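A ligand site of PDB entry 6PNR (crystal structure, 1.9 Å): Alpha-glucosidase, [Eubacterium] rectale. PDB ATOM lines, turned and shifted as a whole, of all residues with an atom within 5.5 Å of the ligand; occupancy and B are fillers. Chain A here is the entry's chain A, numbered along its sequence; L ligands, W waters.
The side-chain hydroxyl (OH) of Tyr 318 sits at hydrogen-bond distance from the side-chain carboxylate (OD2) of Asp 390 (2.6 Å). NH1 of Arg 441 lies within salt-bridge range of OD2 of Asp 458 (3.4 Å). The side-chain carboxylate of Asp 390 lies within salt-bridge range of the guanidinium group of Arg 441 (3.2 Å).
Water W3 lies within hydrogen-bond range of OD2 of Asp 458 (2.4 Å), N1 of the ligand (2.5 Å) and NH1 of Arg 441 (3.4 Å). Water W2 lies within hydrogen-bond range of the side-chain carboxylate (OD2) of Asp 490 (2.6 Å), an oxygen (O4) of the ligand (2.7 Å), the side-chain carboxylate (OD1) of Asp 458 (2.7 Å) and the indole nitrogen (NE1) of Trp 455 (3.1 Å). Water W1 lies within hydrogen-bond range of the side-chain hydroxyl of Tyr 494 (2.6 Å), the backbone carbonyl oxygen of Lys 285 (2.9 Å), an oxygen (O1) of the ligand (3.0 Å) and the side-chain amide nitrogen of Gln 273 (3.4 Å).
Tyr 318 touches the ligand. Phe 391 touches the ligand (CE2 to C3, 3.6 Å). Trp 455 touches the ligand. Tyr 494 touches the ligand. Hydrophobic or aromatic side chains within 4 Å of the ligand: Leu 287, Trp 289, Met 388, Phe 391, Trp 455, Tyr 494 and His 523. Within 4 Å of the ligand: Gln 273, Arg 286, Leu 287, Trp 289, Tyr 318, Met 388, Asp 390, Phe 391, Arg 441, Trp 455, Asp 458, Tyr 494 and His 523.
OD2 of Asp 390 is in salt-bridge range of N1 of the ligand (3.0 Å). A ring nitrogen (NE2) of His 523 is in hydrogen-bond range of an oxygen (O4) of the ligand (3.0 Å). NH2 of Arg 286 lies within salt-bridge range of O2 of the ligand (2.9 Å). The side-chain carboxylate (OD1) of Asp 458 lies within salt-bridge range of a nitrogen (N1) of the ligand, 3.95 Å away. O3 of the ligand is in hydrogen-bond range of N of Leu 287 (3.0 Å). The side-chain amide oxygen of Gln 273 is in hydrogen-bond range of an oxygen (O5) of the ligand. The side-chain sulfur of Met 388 lies close to an oxygen (O4) of the ligand, at 3.5 Å. The indole nitrogen (NE1) of Trp 289 lies within hydrogen-bond range of an oxygen (O3) of the ligand, 3.2 Å away. The guanidinium group (NH1) of Arg 441 lies close to a nitrogen (N1) of the ligand.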
ATOM      1  N   TRP A 271       3.532 -40.661  17.062  1.00  0.00           N
ATOM      2  CA  TRP A 271       2.496 -39.647  16.867  1.00  0.00           C
ATOM      3  C   TRP A 271       2.367 -39.422  15.367  1.00  0.00           C
ATOM      4  O   TRP A 271       3.254 -38.822  14.742  1.00  0.00           O
ATOM      5  CB  TRP A 271       2.846 -38.340  17.590  1.00  0.00           C
ATOM      6  CG  TRP A 271       1.967 -37.211  17.211  1.00  0.00           C
ATOM      7  CD1 TRP A 271       0.593 -37.175  17.276  1.00  0.00           C
ATOM      8  CD2 TRP A 271       2.377 -35.944  16.691  1.00  0.00           C
ATOM      9  NE1 TRP A 271       0.133 -35.956  16.821  1.00  0.00           N
ATOM     10  CE2 TRP A 271       1.205 -35.186  16.449  1.00  0.00           C
ATOM     11  CE3 TRP A 271       3.619 -35.384  16.387  1.00  0.00           C
ATOM     12  CZ2 TRP A 271       1.248 -33.895  15.922  1.00  0.00           C
ATOM     13  CZ3 TRP A 271       3.662 -34.092  15.860  1.00  0.00           C
ATOM     14  CH2 TRP A 271       2.481 -33.373  15.630  1.00  0.00           C
ATOM     15  N   GLN A 273       0.186 -37.514  12.945  1.00  0.00           N
ATOM     16  CA  GLN A 273      -0.883 -36.538  12.808  1.00  0.00           C
ATOM     17  C   GLN A 273      -1.725 -36.775  11.566  1.00  0.00           C
ATOM     18  O   GLN A 273      -2.873 -36.333  11.525  1.00  0.00           O
ATOM     19  CB  GLN A 273      -0.320 -35.110  12.799  1.00  0.00           C
ATOM     20  CG  GLN A 273       0.561 -34.774  11.608  1.00  0.00           C
ATOM     21  CD  GLN A 273       0.782 -33.257  11.480  1.00  0.00           C
ATOM     22  OE1 GLN A 273       0.469 -32.493  12.405  1.00  0.00           O
ATOM     23  NE2 GLN A 273       1.315 -32.821  10.349  1.00  0.00           N
ATOM     24  N   PHE A 283       0.895 -23.973   1.561  1.00  0.00           N
ATOM     25  CA  PHE A 283       1.573 -23.854   2.846  1.00  0.00           C
ATOM     26  C   PHE A 283       2.508 -25.033   3.094  1.00  0.00           C
ATOM     27  O   PHE A 283       3.622 -24.854   3.618  1.00  0.00           O
ATOM     28  CB  PHE A 283       0.542 -23.715   3.971  1.00  0.00           C
ATOM     29  CG  PHE A 283       1.125 -23.573   5.370  1.00  0.00           C
ATOM     30  CD1 PHE A 283       1.815 -22.427   5.745  1.00  0.00           C
ATOM     31  CD2 PHE A 283       0.911 -24.559   6.344  1.00  0.00           C
ATOM     32  CE1 PHE A 283       2.306 -22.290   7.035  1.00  0.00           C
ATOM     33  CE2 PHE A 283       1.406 -24.430   7.630  1.00  0.00           C
ATOM     34  CZ  PHE A 283       2.106 -23.290   7.979  1.00  0.00           C
ATOM     35  N   LYS A 285       2.546 -29.689   3.656  1.00  0.00           N
ATOM     36  CA  LYS A 285       1.830 -30.944   3.841  1.00  0.00           C
ATOM     37  C   LYS A 285       0.935 -30.800   5.075  1.00  0.00           C
ATOM     38  O   LYS A 285       1.419 -30.812   6.211  1.00  0.00           O
ATOM     39  CB  LYS A 285       2.803 -32.101   3.953  1.00  0.00           C
ATOM     40  CG  LYS A 285       2.145 -33.481   3.871  1.00  0.00           C
ATOM     41  CD  LYS A 285       3.169 -34.612   3.919  1.00  0.00           C
ATOM     42  CE  LYS A 285       3.994 -34.707   2.618  1.00  0.00           C
ATOM     43  NZ  LYS A 285       5.401 -35.166   2.887  1.00  0.00           N
ATOM     44  N   ARG A 286      -0.360 -30.614   4.860  1.00  0.00           N
ATOM     45  CA  ARG A 286      -1.306 -30.502   5.960  1.00  0.00           C
ATOM     46  C   ARG A 286      -2.119 -31.793   6.064  1.00  0.00           C
ATOM     47  O   ARG A 286      -1.710 -32.857   5.546  1.00  0.00           O
ATOM     48  CB  ARG A 286      -2.164 -29.243   5.760  1.00  0.00           C
ATOM     49  CG  ARG A 286      -1.325 -28.003   5.431  1.00  0.00           C
ATOM     50  CD  ARG A 286      -2.143 -26.703   5.474  1.00  0.00           C
ATOM     51  NE  ARG A 286      -2.712 -26.480   6.786  1.00  0.00           N
ATOM     52  CZ  ARG A 286      -3.400 -25.398   7.146  1.00  0.00           C
ATOM     53  NH1 ARG A 286      -3.600 -24.422   6.271  1.00  0.00           N
ATOM     54  NH2 ARG A 286      -3.874 -25.295   8.380  1.00  0.00           N
ATOM     55  N   LEU A 287      -3.268 -31.722   6.732  1.00  0.00           N
ATOM     56  CA  LEU A 287      -4.045 -32.867   7.139  1.00  0.00           C
ATOM     57  C   LEU A 287      -5.455 -32.792   6.569  1.00  0.00           C
ATOM     58  O   LEU A 287      -5.970 -31.698   6.306  1.00  0.00           O
ATOM     59  CB  LEU A 287      -4.156 -32.961   8.662  1.00  0.00           C
ATOM     60  CG  LEU A 287      -2.838 -32.968   9.430  1.00  0.00           C
ATOM     61  CD1 LEU A 287      -3.092 -33.011  10.943  1.00  0.00           C
ATOM     62  CD2 LEU A 287      -2.060 -34.182   8.939  1.00  0.00           C
ATOM     63  N   TRP A 289      -9.182 -32.904   7.468  1.00  0.00           N
ATOM     64  CA  TRP A 289      -9.880 -32.643   8.741  1.00  0.00           C
ATOM     65  C   TRP A 289     -11.213 -33.401   8.779  1.00  0.00           C
ATOM     66  O   TRP A 289     -12.309 -32.855   8.625  1.00  0.00           O
ATOM     67  CB  TRP A 289     -10.077 -31.144   8.949  1.00  0.00           C
ATOM     68  CG  TRP A 289      -8.770 -30.388   9.139  1.00  0.00           C
ATOM     69  CD1 TRP A 289      -7.508 -30.903   9.039  1.00  0.00           C
ATOM     70  CD2 TRP A 289      -8.613 -29.006   9.462  1.00  0.00           C
ATOM     71  NE1 TRP A 289      -6.575 -29.916   9.259  1.00  0.00           N
ATOM     72  CE2 TRP A 289      -7.233 -28.743   9.533  1.00  0.00           C
ATOM     73  CE3 TRP A 289      -9.513 -27.955   9.707  1.00  0.00           C
ATOM     74  CZ2 TRP A 289      -6.724 -27.494   9.836  1.00  0.00           C
ATOM     75  CZ3 TRP A 289      -9.013 -26.705   9.998  1.00  0.00           C
ATOM     76  CH2 TRP A 289      -7.625 -26.487  10.066  1.00  0.00           C
ATOM     77  N   TYR A 318      -4.564 -36.946  16.213  1.00  0.00           N
ATOM     78  CA  TYR A 318      -4.794 -35.518  16.033  1.00  0.00           C
ATOM     79  C   TYR A 318      -6.281 -35.292  15.801  1.00  0.00           C
ATOM     80  O   TYR A 318      -6.883 -36.016  15.014  1.00  0.00           O
ATOM     81  CB  TYR A 318      -3.973 -34.998  14.819  1.00  0.00           C
ATOM     82  CG  TYR A 318      -4.240 -33.552  14.454  1.00  0.00           C
ATOM     83  CD1 TYR A 318      -5.413 -33.173  13.810  1.00  0.00           C
ATOM     84  CD2 TYR A 318      -3.308 -32.561  14.757  1.00  0.00           C
ATOM     85  CE1 TYR A 318      -5.669 -31.867  13.502  1.00  0.00           C
ATOM     86  CE2 TYR A 318      -3.546 -31.239  14.436  1.00  0.00           C
ATOM     87  CZ  TYR A 318      -4.743 -30.898  13.816  1.00  0.00           C
ATOM     88  OH  TYR A 318      -5.025 -29.585  13.466  1.00  0.00           O
ATOM     89  N   PHE A 355      -8.719 -24.485   1.732  1.00  0.00           N
ATOM     90  CA  PHE A 355      -9.809 -25.403   2.031  1.00  0.00           C
ATOM     91  C   PHE A 355     -10.703 -24.744   3.077  1.00  0.00           C
ATOM     92  O   PHE A 355     -10.269 -23.863   3.823  1.00  0.00           O
ATOM     93  CB  PHE A 355      -9.301 -26.792   2.494  1.00  0.00           C
ATOM     94  CG  PHE A 355      -8.481 -26.792   3.771  1.00  0.00           C
ATOM     95  CD1 PHE A 355      -7.117 -26.507   3.740  1.00  0.00           C
ATOM     96  CD2 PHE A 355      -9.050 -27.167   4.983  1.00  0.00           C
ATOM     97  CE1 PHE A 355      -6.348 -26.548   4.900  1.00  0.00           C
ATOM     98  CE2 PHE A 355      -8.286 -27.205   6.156  1.00  0.00           C
ATOM     99  CZ  PHE A 355      -6.935 -26.906   6.110  1.00  0.00           C
ATOM    100  N   MET A 388      -2.779 -34.712  19.591  1.00  0.00           N
ATOM    101  CA  MET A 388      -2.782 -33.266  19.497  1.00  0.00           C
ATOM    102  C   MET A 388      -4.224 -32.798  19.381  1.00  0.00           C
ATOM    103  O   MET A 388      -4.960 -33.258  18.511  1.00  0.00           O
ATOM    104  CB  MET A 388      -1.971 -32.804  18.284  1.00  0.00           C
ATOM    105  CG  MET A 388      -1.928 -31.290  18.115  1.00  0.00           C
ATOM    106  SD  MET A 388      -0.852 -30.745  16.749  1.00  0.00           S
ATOM    107  CE  MET A 388       0.760 -30.900  17.486  1.00  0.00           C
ATOM    108  N   ASP A 390      -5.921 -29.595  18.578  1.00  0.00           N
ATOM    109  CA  ASP A 390      -5.331 -28.422  17.951  1.00  0.00           C
ATOM    110  C   ASP A 390      -6.362 -27.304  17.781  1.00  0.00           C
ATOM    111  O   ASP A 390      -7.566 -27.498  17.950  1.00  0.00           O
ATOM    112  CB  ASP A 390      -4.764 -28.850  16.592  1.00  0.00           C
ATOM    113  CG  ASP A 390      -3.789 -27.858  16.021  1.00  0.00           C
ATOM    114  OD1 ASP A 390      -3.366 -26.879  16.696  1.00  0.00           O
ATOM    115  OD2 ASP A 390      -3.455 -28.064  14.851  1.00  0.00           O
ATOM    116  N   PHE A 391      -5.850 -26.130  17.441  1.00  0.00           N
ATOM    117  CA  PHE A 391      -6.639 -24.958  17.078  1.00  0.00           C
ATOM    118  C   PHE A 391      -7.581 -24.519  18.192  1.00  0.00           C
ATOM    119  O   PHE A 391      -7.366 -24.823  19.372  1.00  0.00           O
ATOM    120  CB  PHE A 391      -7.413 -25.219  15.789  1.00  0.00           C
ATOM    121  CG  PHE A 391      -6.552 -25.197  14.545  1.00  0.00           C
ATOM    122  CD1 PHE A 391      -6.253 -23.997  13.915  1.00  0.00           C
ATOM    123  CD2 PHE A 391      -6.036 -26.372  14.012  1.00  0.00           C
ATOM    124  CE1 PHE A 391      -5.461 -23.970  12.752  1.00  0.00           C
ATOM    125  CE2 PHE A 391      -5.244 -26.350  12.858  1.00  0.00           C
ATOM    126  CZ  PHE A 391      -4.945 -25.154  12.237  1.00  0.00           C
ATOM    127  N   ARG A 441      -2.559 -26.146  22.082  1.00  0.00           N
ATOM    128  CA  ARG A 441      -1.809 -24.916  21.977  1.00  0.00           C
ATOM    129  C   ARG A 441      -2.638 -23.679  22.329  1.00  0.00           C
ATOM    130  O   ARG A 441      -2.071 -22.678  22.767  1.00  0.00           O
ATOM    131  CB  ARG A 441      -1.238 -24.754  20.551  1.00  0.00           C
ATOM    132  CG  ARG A 441      -2.311 -24.555  19.485  1.00  0.00           C
ATOM    133  CD  ARG A 441      -1.717 -24.349  18.073  1.00  0.00           C
ATOM    134  NE  ARG A 441      -2.704 -23.789  17.158  1.00  0.00           N
ATOM    135  CZ  ARG A 441      -2.497 -23.538  15.866  1.00  0.00           C
ATOM    136  NH1 ARG A 441      -1.313 -23.794  15.312  1.00  0.00           N
ATOM    137  NH2 ARG A 441      -3.470 -23.016  15.125  1.00  0.00           N
ATOM    138  N   TRP A 455       1.242 -27.351  24.696  1.00  0.00           N
ATOM    139  CA  TRP A 455       2.492 -27.199  23.963  1.00  0.00           C
ATOM    140  C   TRP A 455       2.528 -25.774  23.419  1.00  0.00           C
ATOM    141  O   TRP A 455       1.501 -25.106  23.279  1.00  0.00           O
ATOM    142  CB  TRP A 455       2.693 -28.282  22.875  1.00  0.00           C
ATOM    143  CG  TRP A 455       2.408 -27.933  21.430  1.00  0.00           C
ATOM    144  CD1 TRP A 455       3.317 -27.547  20.476  1.00  0.00           C
ATOM    145  CD2 TRP A 455       1.145 -28.034  20.752  1.00  0.00           C
ATOM    146  NE1 TRP A 455       2.694 -27.371  19.270  1.00  0.00           N
ATOM    147  CE2 TRP A 455       1.359 -27.659  19.404  1.00  0.00           C
ATOM    148  CE3 TRP A 455      -0.151 -28.403  21.163  1.00  0.00           C
ATOM    149  CZ2 TRP A 455       0.318 -27.617  18.468  1.00  0.00           C
ATOM    150  CZ3 TRP A 455      -1.175 -28.378  20.229  1.00  0.00           C
ATOM    151  CH2 TRP A 455      -0.930 -27.980  18.896  1.00  0.00           C
ATOM    152  N   ASP A 458       3.124 -23.295  17.247  1.00  0.00           N
ATOM    153  CA  ASP A 458       4.059 -23.286  16.124  1.00  0.00           C
ATOM    154  C   ASP A 458       5.166 -22.270  16.354  1.00  0.00           C
ATOM    155  O   ASP A 458       4.906 -21.064  16.427  1.00  0.00           O
ATOM    156  CB  ASP A 458       3.341 -22.907  14.823  1.00  0.00           C
ATOM    157  CG  ASP A 458       2.206 -23.843  14.442  1.00  0.00           C
ATOM    158  OD1 ASP A 458       2.025 -24.907  15.085  1.00  0.00           O
ATOM    159  OD2 ASP A 458       1.514 -23.508  13.452  1.00  0.00           O
ATOM    160  N   ASP A 490       7.403 -28.498  20.038  1.00  0.00           N
ATOM    161  CA  ASP A 490       7.900 -29.262  18.887  1.00  0.00           C
ATOM    162  C   ASP A 490       9.425 -29.238  18.872  1.00  0.00           C
ATOM    163  O   ASP A 490      10.018 -28.171  18.691  1.00  0.00           O
ATOM    164  CB  ASP A 490       7.409 -28.641  17.570  1.00  0.00           C
ATOM    165  CG  ASP A 490       5.892 -28.545  17.447  1.00  0.00           C
ATOM    166  OD1 ASP A 490       5.201 -29.488  17.880  1.00  0.00           O
ATOM    167  OD2 ASP A 490       5.409 -27.544  16.879  1.00  0.00           O
ATOM    168  N   TYR A 494       8.322 -25.772  13.981  1.00  0.00           N
ATOM    169  CA  TYR A 494       7.306 -26.204  13.027  1.00  0.00           C
ATOM    170  C   TYR A 494       7.403 -25.437  11.705  1.00  0.00           C
ATOM    171  O   TYR A 494       7.493 -26.067  10.655  1.00  0.00           O
ATOM    172  CB  TYR A 494       5.892 -26.031  13.608  1.00  0.00           C
ATOM    173  CG  TYR A 494       4.812 -26.374  12.588  1.00  0.00           C
ATOM    174  CD1 TYR A 494       4.471 -27.708  12.334  1.00  0.00           C
ATOM    175  CD2 TYR A 494       4.140 -25.370  11.889  1.00  0.00           C
ATOM    176  CE1 TYR A 494       3.492 -28.027  11.399  1.00  0.00           C
ATOM    177  CE2 TYR A 494       3.143 -25.683  10.969  1.00  0.00           C
ATOM    178  CZ  TYR A 494       2.833 -27.008  10.709  1.00  0.00           C
ATOM    179  OH  TYR A 494       1.868 -27.317   9.792  1.00  0.00           O
ATOM    180  N   HIS A 523       8.484 -33.320  15.426  1.00  0.00           N
ATOM    181  CA  HIS A 523       7.456 -32.913  14.491  1.00  0.00           C
ATOM    182  C   HIS A 523       8.110 -32.749  13.126  1.00  0.00           C
ATOM    183  O   HIS A 523       9.166 -32.123  13.039  1.00  0.00           O
ATOM    184  CB  HIS A 523       6.804 -31.587  14.957  1.00  0.00           C
ATOM    185  CG  HIS A 523       5.492 -31.271  14.308  1.00  0.00           C
ATOM    186  ND1 HIS A 523       5.182 -31.647  13.012  1.00  0.00           N
ATOM    187  CD2 HIS A 523       4.426 -30.572  14.761  1.00  0.00           C
ATOM    188  CE1 HIS A 523       3.962 -31.215  12.709  1.00  0.00           C
ATOM    189  NE2 HIS A 523       3.484 -30.560  13.752  1.00  0.00           N
HETATM  190  O1  LIG L   1      -1.433 -28.619   8.764  1.00  0.00           O
HETATM  191  S1  LIG L   1      -2.558 -28.854   9.661  1.00  0.00           S
HETATM  192  O2  LIG L   1      -3.230 -27.614   9.962  1.00  0.00           O
HETATM  193  O3  LIG L   1      -3.424 -29.899   9.155  1.00  0.00           O
HETATM  194  C1  LIG L   1      -1.820 -29.458  11.156  1.00  0.00           C
HETATM  195  C2  LIG L   1      -0.937 -28.440  11.889  1.00  0.00           C
HETATM  196  C3  LIG L   1      -1.838 -27.424  12.562  1.00  0.00           C
HETATM  197  N1  LIG L   1      -1.238 -26.531  13.550  1.00  0.00           N
HETATM  198  C4  LIG L   1      -0.447 -27.262  14.547  1.00  0.00           C
HETATM  199  C5  LIG L   1       0.603 -28.118  13.854  1.00  0.00           C
HETATM  200  O4  LIG L   1       1.340 -28.809  14.861  1.00  0.00           O
HETATM  201  C6  LIG L   1      -0.066 -29.128  12.935  1.00  0.00           C
HETATM  202  O5  LIG L   1       0.907 -29.943  12.298  1.00  0.00           O
HETATM  203  O   HOH W   1       1.333 -29.727   8.951  1.00  0.00           O
HETATM  204  O   HOH W   2       2.934 -27.166  16.212  1.00  0.00           O
HETATM  205  O   HOH W   3      -0.273 -24.630  12.209  1.00  0.00           O
